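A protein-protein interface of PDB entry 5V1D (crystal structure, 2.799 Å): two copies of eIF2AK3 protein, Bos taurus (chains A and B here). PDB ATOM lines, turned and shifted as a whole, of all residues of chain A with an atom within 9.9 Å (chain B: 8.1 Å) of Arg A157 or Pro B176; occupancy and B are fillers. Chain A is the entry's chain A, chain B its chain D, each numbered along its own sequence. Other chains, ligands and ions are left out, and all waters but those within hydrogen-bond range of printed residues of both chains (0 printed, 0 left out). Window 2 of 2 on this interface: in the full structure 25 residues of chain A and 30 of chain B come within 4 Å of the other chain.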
ATOM      1  N   ASP A  97     -25.768  22.929  -3.747  1.00  0.00           N
ATOM      2  CA  ASP A  97     -25.301  23.726  -2.620  1.00  0.00           C
ATOM      3  C   ASP A  97     -23.972  23.193  -2.084  1.00  0.00           C
ATOM      4  O   ASP A  97     -23.083  23.973  -1.742  1.00  0.00           O
ATOM      5  CB  ASP A  97     -26.354  23.751  -1.505  1.00  0.00           C
ATOM      6  CG  ASP A  97     -26.022  24.748  -0.392  1.00  0.00           C
ATOM      7  OD1 ASP A  97     -24.965  24.610   0.261  1.00  0.00           O
ATOM      8  OD2 ASP A  97     -26.830  25.676  -0.168  1.00  0.00           O
ATOM      9  N   VAL A  98     -23.837  21.870  -2.012  1.00  0.00           N
ATOM     10  CA  VAL A  98     -22.646  21.269  -1.420  1.00  0.00           C
ATOM     11  C   VAL A  98     -22.430  19.888  -2.023  1.00  0.00           C
ATOM     12  O   VAL A  98     -23.281  19.389  -2.766  1.00  0.00           O
ATOM     13  CB  VAL A  98     -22.769  21.200   0.118  1.00  0.00           C
ATOM     14  CG1 VAL A  98     -23.607  20.004   0.536  1.00  0.00           C
ATOM     15  CG2 VAL A  98     -21.400  21.168   0.777  1.00  0.00           C
ATOM     16  N   VAL A  99     -21.289  19.272  -1.730  1.00  0.00           N
ATOM     17  CA  VAL A  99     -21.009  17.895  -2.115  1.00  0.00           C
ATOM     18  C   VAL A  99     -20.512  17.151  -0.886  1.00  0.00           C
ATOM     19  O   VAL A  99     -19.641  17.648  -0.162  1.00  0.00           O
ATOM     20  CB  VAL A  99     -19.986  17.815  -3.261  1.00  0.00           C
ATOM     21  CG1 VAL A  99     -19.349  16.437  -3.323  1.00  0.00           C
ATOM     22  CG2 VAL A  99     -20.671  18.136  -4.569  1.00  0.00           C
ATOM     23  N   VAL A 154     -18.186  19.426   1.018  1.00  0.00           N
ATOM     24  CA  VAL A 154     -17.125  19.982   0.187  1.00  0.00           C
ATOM     25  C   VAL A 154     -17.745  20.751  -0.973  1.00  0.00           C
ATOM     26  O   VAL A 154     -18.693  20.279  -1.609  1.00  0.00           O
ATOM     27  CB  VAL A 154     -16.177  18.875  -0.320  1.00  0.00           C
ATOM     28  CG1 VAL A 154     -15.468  19.309  -1.592  1.00  0.00           C
ATOM     29  CG2 VAL A 154     -15.167  18.513   0.757  1.00  0.00           C
ATOM     30  N   GLY A 155     -17.211  21.946  -1.232  1.00  0.00           N
ATOM     31  CA  GLY A 155     -17.653  22.774  -2.326  1.00  0.00           C
ATOM     32  C   GLY A 155     -17.373  22.129  -3.664  1.00  0.00           C
ATOM     33  O   GLY A 155     -16.306  21.550  -3.889  1.00  0.00           O
ATOM     34  N   PRO A 156     -18.334  22.225  -4.586  1.00  0.00           N
ATOM     35  CA  PRO A 156     -18.231  21.445  -5.828  1.00  0.00           C
ATOM     36  C   PRO A 156     -17.098  21.886  -6.728  1.00  0.00           C
ATOM     37  O   PRO A 156     -16.509  21.042  -7.414  1.00  0.00           O
ATOM     38  CB  PRO A 156     -19.597  21.665  -6.496  1.00  0.00           C
ATOM     39  CG  PRO A 156     -20.491  22.179  -5.407  1.00  0.00           C
ATOM     40  CD  PRO A 156     -19.602  22.965  -4.505  1.00  0.00           C
ATOM     41  N   ARG A 157     -16.775  23.176  -6.748  1.00  0.00           N
ATOM     42  CA  ARG A 157     -15.768  23.725  -7.647  1.00  0.00           C
ATOM     43  C   ARG A 157     -14.391  23.834  -7.011  1.00  0.00           C
ATOM     44  O   ARG A 157     -13.389  23.533  -7.666  1.00  0.00           O
ATOM     45  CB  ARG A 157     -16.213  25.104  -8.150  1.00  0.00           C
ATOM     46  CG  ARG A 157     -15.084  25.966  -8.691  1.00  0.00           C
ATOM     47  CD  ARG A 157     -15.491  26.707  -9.957  1.00  0.00           C
ATOM     48  NE  ARG A 157     -15.075  25.996 -11.164  1.00  0.00           N
ATOM     49  CZ  ARG A 157     -15.427  26.349 -12.398  1.00  0.00           C
ATOM     50  NH1 ARG A 157     -16.213  27.399 -12.590  1.00  0.00           N
ATOM     51  NH2 ARG A 157     -14.999  25.647 -13.439  1.00  0.00           N
ATOM     52  N   SER A 158     -14.316  24.243  -5.745  1.00  0.00           N
ATOM     53  CA  SER A 158     -13.025  24.428  -5.089  1.00  0.00           C
ATOM     54  C   SER A 158     -12.468  23.116  -4.548  1.00  0.00           C
ATOM     55  O   SER A 158     -11.312  22.769  -4.814  1.00  0.00           O
ATOM     56  CB  SER A 158     -13.156  25.454  -3.964  1.00  0.00           C
ATOM     57  OG  SER A 158     -14.198  25.097  -3.075  1.00  0.00           O
ATOM     58  N   GLY A 159     -13.263  22.385  -3.773  1.00  0.00           N
ATOM     59  CA  GLY A 159     -12.809  21.153  -3.163  1.00  0.00           C
ATOM     60  C   GLY A 159     -12.263  21.284  -1.756  1.00  0.00           C
ATOM     61  O   GLY A 159     -11.806  20.280  -1.197  1.00  0.00           O
ATOM     62  N   ASN A 160     -12.292  22.478  -1.170  1.00  0.00           N
ATOM     63  CA  ASN A 160     -11.823  22.669   0.195  1.00  0.00           C
ATOM     64  C   ASN A 160     -12.925  22.313   1.186  1.00  0.00           C
ATOM     65  O   ASN A 160     -14.116  22.412   0.879  1.00  0.00           O
ATOM     66  CB  ASN A 160     -11.374  24.115   0.413  1.00  0.00           C
ATOM     67  CG  ASN A 160     -10.539  24.651  -0.738  1.00  0.00           C
ATOM     68  OD1 ASN A 160      -9.864  23.895  -1.439  1.00  0.00           O
ATOM     69  ND2 ASN A 160     -10.586  25.963  -0.940  1.00  0.00           N
ATOM     70  N   GLU A 161     -12.519  21.901   2.386  1.00  0.00           N
ATOM     71  CA  GLU A 161     -13.489  21.452   3.378  1.00  0.00           C
ATOM     72  C   GLU A 161     -14.466  22.569   3.738  1.00  0.00           C
ATOM     73  O   GLU A 161     -14.108  23.749   3.766  1.00  0.00           O
ATOM     74  CB  GLU A 161     -12.782  20.956   4.644  1.00  0.00           C
ATOM     75  CG  GLU A 161     -12.042  19.634   4.498  1.00  0.00           C
ATOM     76  CD  GLU A 161     -11.373  19.202   5.792  1.00  0.00           C
ATOM     77  OE1 GLU A 161     -11.486  19.943   6.789  1.00  0.00           O
ATOM     78  OE2 GLU A 161     -10.736  18.127   5.816  1.00  0.00           O
ATOM     79  N   GLY B 110     -12.998  15.797  -8.736  1.00  0.00           N
ATOM     80  CA  GLY B 110     -13.419  16.924  -9.537  1.00  0.00           C
ATOM     81  C   GLY B 110     -12.485  17.144 -10.711  1.00  0.00           C
ATOM     82  O   GLY B 110     -11.292  17.393 -10.528  1.00  0.00           O
ATOM     83  N   LEU B 111     -13.040  17.054 -11.917  1.00  0.00           N
ATOM     84  CA  LEU B 111     -12.268  17.170 -13.145  1.00  0.00           C
ATOM     85  C   LEU B 111     -12.717  18.380 -13.948  1.00  0.00           C
ATOM     86  O   LEU B 111     -13.890  18.763 -13.921  1.00  0.00           O
ATOM     87  CB  LEU B 111     -12.425  15.933 -14.018  1.00  0.00           C
ATOM     88  CG  LEU B 111     -12.477  14.597 -13.299  1.00  0.00           C
ATOM     89  CD1 LEU B 111     -12.644  13.502 -14.326  1.00  0.00           C
ATOM     90  CD2 LEU B 111     -11.216  14.403 -12.499  1.00  0.00           C
ATOM     91  N   SER B 112     -11.775  18.965 -14.680  1.00  0.00           N
ATOM     92  CA  SER B 112     -12.120  20.030 -15.609  1.00  0.00           C
ATOM     93  C   SER B 112     -13.070  19.505 -16.674  1.00  0.00           C
ATOM     94  O   SER B 112     -12.868  18.418 -17.223  1.00  0.00           O
ATOM     95  CB  SER B 112     -10.863  20.581 -16.266  1.00  0.00           C
ATOM     96  OG  SER B 112     -10.192  19.540 -16.950  1.00  0.00           O
ATOM     97  N   ALA B 113     -14.106  20.293 -16.969  1.00  0.00           N
ATOM     98  CA  ALA B 113     -15.164  19.827 -17.859  1.00  0.00           C
ATOM     99  C   ALA B 113     -14.605  19.366 -19.198  1.00  0.00           C
ATOM    100  O   ALA B 113     -15.074  18.371 -19.762  1.00  0.00           O
ATOM    101  CB  ALA B 113     -16.201  20.930 -18.063  1.00  0.00           C
ATOM    102  N   ARG B 119      -8.989  18.479 -10.840  1.00  0.00           N
ATOM    103  CA  ARG B 119      -8.920  19.728 -10.096  1.00  0.00           C
ATOM    104  C   ARG B 119      -8.823  19.472  -8.602  1.00  0.00           C
ATOM    105  O   ARG B 119      -8.099  20.179  -7.895  1.00  0.00           O
ATOM    106  CB  ARG B 119     -10.128  20.603 -10.424  1.00  0.00           C
ATOM    107  CG  ARG B 119     -10.048  21.234 -11.807  1.00  0.00           C
ATOM    108  CD  ARG B 119      -8.660  21.815 -12.038  1.00  0.00           C
ATOM    109  NE  ARG B 119      -8.444  22.248 -13.413  1.00  0.00           N
ATOM    110  CZ  ARG B 119      -7.248  22.517 -13.924  1.00  0.00           C
ATOM    111  NH1 ARG B 119      -6.163  22.391 -13.173  1.00  0.00           N
ATOM    112  NH2 ARG B 119      -7.136  22.905 -15.189  1.00  0.00           N
ATOM    113  N   TYR B 120      -9.528  18.459  -8.109  1.00  0.00           N
ATOM    114  CA  TYR B 120      -9.404  18.059  -6.717  1.00  0.00           C
ATOM    115  C   TYR B 120      -9.913  16.640  -6.561  1.00  0.00           C
ATOM    116  O   TYR B 120     -10.705  16.148  -7.367  1.00  0.00           O
ATOM    117  CB  TYR B 120     -10.175  18.986  -5.777  1.00  0.00           C
ATOM    118  CG  TYR B 120     -11.683  18.944  -5.938  1.00  0.00           C
ATOM    119  CD1 TYR B 120     -12.346  19.955  -6.612  1.00  0.00           C
ATOM    120  CD2 TYR B 120     -12.447  17.912  -5.394  1.00  0.00           C
ATOM    121  CE1 TYR B 120     -13.720  19.940  -6.756  1.00  0.00           C
ATOM    122  CE2 TYR B 120     -13.826  17.888  -5.535  1.00  0.00           C
ATOM    123  CZ  TYR B 120     -14.454  18.908  -6.220  1.00  0.00           C
ATOM    124  OH  TYR B 120     -15.819  18.918  -6.376  1.00  0.00           O
ATOM    125  N   GLN B 129      -6.035  19.633  -3.405  1.00  0.00           N
ATOM    126  CA  GLN B 129      -6.416  20.524  -4.493  1.00  0.00           C
ATOM    127  C   GLN B 129      -5.207  20.842  -5.358  1.00  0.00           C
ATOM    128  O   GLN B 129      -4.080  20.940  -4.867  1.00  0.00           O
ATOM    129  CB  GLN B 129      -7.023  21.827  -3.968  1.00  0.00           C
ATOM    130  CG  GLN B 129      -8.093  21.641  -2.912  1.00  0.00           C
ATOM    131  CD  GLN B 129      -7.509  21.505  -1.531  1.00  0.00           C
ATOM    132  OE1 GLN B 129      -6.411  20.979  -1.357  1.00  0.00           O
ATOM    133  NE2 GLN B 129      -8.232  21.996  -0.535  1.00  0.00           N
ATOM    134  N   ASP B 140     -16.437  24.140 -17.468  1.00  0.00           N
ATOM    135  CA  ASP B 140     -16.847  24.117 -16.071  1.00  0.00           C
ATOM    136  C   ASP B 140     -16.172  22.967 -15.354  1.00  0.00           C
ATOM    137  O   ASP B 140     -14.969  22.757 -15.514  1.00  0.00           O
ATOM    138  CB  ASP B 140     -18.362  24.000 -15.952  1.00  0.00           C
ATOM    139  CG  ASP B 140     -19.079  25.092 -16.697  1.00  0.00           C
ATOM    140  OD1 ASP B 140     -19.511  24.844 -17.843  1.00  0.00           O
ATOM    141  OD2 ASP B 140     -19.183  26.209 -16.145  1.00  0.00           O
ATOM    142  N   ILE B 141     -16.951  22.208 -14.583  1.00  0.00           N
ATOM    143  CA  ILE B 141     -16.420  21.156 -13.721  1.00  0.00           C
ATOM    144  C   ILE B 141     -17.182  19.862 -13.963  1.00  0.00           C
ATOM    145  O   ILE B 141     -18.418  19.850 -13.961  1.00  0.00           O
ATOM    146  CB  ILE B 141     -16.496  21.543 -12.231  1.00  0.00           C
ATOM    147  CG1 ILE B 141     -15.375  22.512 -11.864  1.00  0.00           C
ATOM    148  CG2 ILE B 141     -16.406  20.307 -11.349  1.00  0.00           C
ATOM    149  CD1 ILE B 141     -14.018  21.847 -11.742  1.00  0.00           C
ATOM    150  N   LEU B 142     -16.441  18.776 -14.165  1.00  0.00           N
ATOM    151  CA  LEU B 142     -16.977  17.425 -14.112  1.00  0.00           C
ATOM    152  C   LEU B 142     -16.759  16.860 -12.717  1.00  0.00           C
ATOM    153  O   LEU B 142     -15.634  16.879 -12.206  1.00  0.00           O
ATOM    154  CB  LEU B 142     -16.303  16.524 -15.143  1.00  0.00           C
ATOM    155  CG  LEU B 142     -16.804  16.681 -16.567  1.00  0.00           C
ATOM    156  CD1 LEU B 142     -16.079  15.697 -17.459  1.00  0.00           C
ATOM    157  CD2 LEU B 142     -18.304  16.459 -16.606  1.00  0.00           C
ATOM    158  N   LEU B 143     -17.823  16.348 -12.113  1.00  0.00           N
ATOM    159  CA  LEU B 143     -17.783  15.822 -10.756  1.00  0.00           C
ATOM    160  C   LEU B 143     -17.974  14.313 -10.795  1.00  0.00           C
ATOM    161  O   LEU B 143     -19.020  13.830 -11.238  1.00  0.00           O
ATOM    162  CB  LEU B 143     -18.862  16.474  -9.896  1.00  0.00           C
ATOM    163  CG  LEU B 143     -18.870  16.118  -8.416  1.00  0.00           C
ATOM    164  CD1 LEU B 143     -17.749  16.829  -7.686  1.00  0.00           C
ATOM    165  CD2 LEU B 143     -20.212  16.481  -7.831  1.00  0.00           C
ATOM    166  N   ARG B 173     -21.906  13.882 -12.463  1.00  0.00           N
ATOM    167  CA  ARG B 173     -22.710  15.094 -12.497  1.00  0.00           C
ATOM    168  C   ARG B 173     -21.844  16.251 -12.969  1.00  0.00           C
ATOM    169  O   ARG B 173     -20.614  16.179 -12.953  1.00  0.00           O
ATOM    170  CB  ARG B 173     -23.326  15.404 -11.132  1.00  0.00           C
ATOM    171  CG  ARG B 173     -24.660  14.724 -10.896  1.00  0.00           C
ATOM    172  CD  ARG B 173     -24.812  14.347  -9.441  1.00  0.00           C
ATOM    173  NE  ARG B 173     -23.730  13.463  -9.023  1.00  0.00           N
ATOM    174  CZ  ARG B 173     -23.761  12.143  -9.155  1.00  0.00           C
ATOM    175  NH1 ARG B 173     -24.827  11.556  -9.687  1.00  0.00           N
ATOM    176  NH2 ARG B 173     -22.730  11.412  -8.755  1.00  0.00           N
ATOM    177  N   TYR B 174     -22.503  17.327 -13.389  1.00  0.00           N
ATOM    178  CA  TYR B 174     -21.836  18.479 -13.975  1.00  0.00           C
ATOM    179  C   TYR B 174     -21.988  19.688 -13.065  1.00  0.00           C
ATOM    180  O   TYR B 174     -23.047  19.894 -12.460  1.00  0.00           O
ATOM    181  CB  TYR B 174     -22.408  18.791 -15.355  1.00  0.00           C
ATOM    182  CG  TYR B 174     -21.550  19.705 -16.188  1.00  0.00           C
ATOM    183  CD1 TYR B 174     -20.542  19.194 -16.992  1.00  0.00           C
ATOM    184  CD2 TYR B 174     -21.756  21.076 -16.185  1.00  0.00           C
ATOM    185  CE1 TYR B 174     -19.753  20.025 -17.769  1.00  0.00           C
ATOM    186  CE2 TYR B 174     -20.976  21.915 -16.960  1.00  0.00           C
ATOM    187  CZ  TYR B 174     -19.974  21.383 -17.747  1.00  0.00           C
ATOM    188  OH  TYR B 174     -19.194  22.216 -18.512  1.00  0.00           O
ATOM    189  N   ILE B 175     -20.930  20.487 -12.978  1.00  0.00           N
ATOM    190  CA  ILE B 175     -20.907  21.637 -12.076  1.00  0.00           C
ATOM    191  C   ILE B 175     -20.520  22.899 -12.837  1.00  0.00           C
ATOM    192  O   ILE B 175     -19.326  23.151 -13.049  1.00  0.00           O
ATOM    193  CB  ILE B 175     -19.935  21.414 -10.912  1.00  0.00           C
ATOM    194  CG1 ILE B 175     -20.231  20.094 -10.195  1.00  0.00           C
ATOM    195  CG2 ILE B 175     -19.995  22.595  -9.959  1.00  0.00           C
ATOM    196  CD1 ILE B 175     -21.600  20.030  -9.569  1.00  0.00           C
ATOM    197  N   PRO B 176     -21.486  23.728 -13.252  1.00  0.00           N
ATOM    198  CA  PRO B 176     -21.191  25.002 -13.916  1.00  0.00           C
ATOM    199  C   PRO B 176     -20.595  26.043 -12.965  1.00  0.00           C
ATOM    200  O   PRO B 176     -19.736  26.831 -13.367  1.00  0.00           O
ATOM    201  CB  PRO B 176     -22.561  25.450 -14.428  1.00  0.00           C
ATOM    202  CG  PRO B 176     -23.533  24.802 -13.508  1.00  0.00           C
ATOM    203  CD  PRO B 176     -22.935  23.473 -13.164  1.00  0.00           C
ATOM    204  N   GLY B 254     -23.483  21.097 -20.792  1.00  0.00           N
ATOM    205  CA  GLY B 254     -23.763  21.148 -19.373  1.00  0.00           C
ATOM    206  C   GLY B 254     -24.528  19.936 -18.892  1.00  0.00           C
ATOM    207  O   GLY B 254     -24.030  19.171 -18.062  1.00  0.00           O
ATOM    208  N   LYS B 255     -25.737  19.751 -19.412  1.00  0.00           N
ATOM    209  CA  LYS B 255     -26.563  18.616 -19.027  1.00  0.00           C
ATOM    210  C   LYS B 255     -25.836  17.300 -19.283  1.00  0.00           C
ATOM    211  O   LYS B 255     -25.143  17.142 -20.290  1.00  0.00           O
ATOM    212  CB  LYS B 255     -27.883  18.672 -19.797  1.00  0.00           C
ATOM    213  CG  LYS B 255     -28.610  17.351 -19.924  1.00  0.00           C
ATOM    214  CD  LYS B 255     -28.503  16.816 -21.346  1.00  0.00           C
ATOM    215  CE  LYS B 255     -29.118  17.772 -22.362  1.00  0.00           C
ATOM    216  NZ  LYS B 255     -28.993  17.262 -23.759  1.00  0.00           N
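Arg A157 touches four residues of chain B. Of chain A, only Arg A157 comes within 4 Å of Pro B176. Asp B140 touches just one residue of chain A: Arg A157. Printed residues of chain B within 4 Å of Ser A158: Tyr B120 and Gln B129. Printed residues of chain A within 4 Å of Gln B129: Ser A158 and Asn A160. Of the printed residues of chain B, Val A99 touches Leu B143 (3.7 Å). The nearest residue of chain B that does not touch Arg A157 is Ile B175 (4.6 Å). The nearest residue of chain A that does not touch Pro B176 is Pro A156 (7.3 Å). The nearest printed residue of chain B that does not touch Pro A156 is Ile B141 (4.004 Å).
OH of Tyr B120 sits at hydrogen-bond distance from O of Pro A156. The side-chain amide oxygen (OD1) of Asn A160 is in hydrogen-bond range of the side-chain amide nitrogen (NE2) of Gln B129.
The backbone NH (N) of Gly B110 sits at hydrogen-bond distance from the backbone carbonyl oxygen (O) of Tyr B120. The backbone carbonyl oxygen (O) of Ile B141 lies within hydrogen-bond range of the backbone NH (N) of Ile B175 (2.8 Å). The backbone NH (N) of Val A154 lies within hydrogen-bond range of the backbone carbonyl oxygen (O) of Val A99, at 2.6 Å. The backbone carbonyl oxygen of Asp B140 sits at hydrogen-bond distance from the backbone NH of Ala B113 (3.0 Å). The side-chain hydroxyl (OH) of Tyr B174 lies within hydrogen-bond range of the side-chain carboxylate (OD1) of Asp B140. The backbone NH (N) of Leu B143 lies within hydrogen-bond range of the backbone carbonyl oxygen (O) of Arg B173.
No position is printed for both chains. Of the 12 pairs that touch across the chains among the printed residues, none has its exchanged pair printed and touching as well.
Among the printed residues, merely in contact across the chains: Val A99 with Leu B143, Gly A155 with Tyr B120, Pro A156 with Ile B175, Arg A157 with Tyr B120, Arg A157 with Asp B140, Arg A157 with Ile B141, Arg A157 with Pro B176, Ser A158 with Tyr B120, Ser A158 with Gln B129 and Gly A159 with Tyr B120.
Of the 17 printed residues of chain B, 7 touch a printed residue of chain A. Printed residues of chain B that touch a printed residue of chain A: Tyr B120, Gln B129, Asp B140, Ile B141, Leu B143, Ile B175 and Pro B176. Hydrophobic or aromatic side chains of chain B that line the printed part of chain A: Tyr B120, Ile B141, Leu B143 and Ile B175. Among the printed residues, 12 pairs touch across the chains. Among the printed residues, no Asp or Glu carboxylate lies within 4 Å of a Lys or Arg side-chain nitrogen of the other chain.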
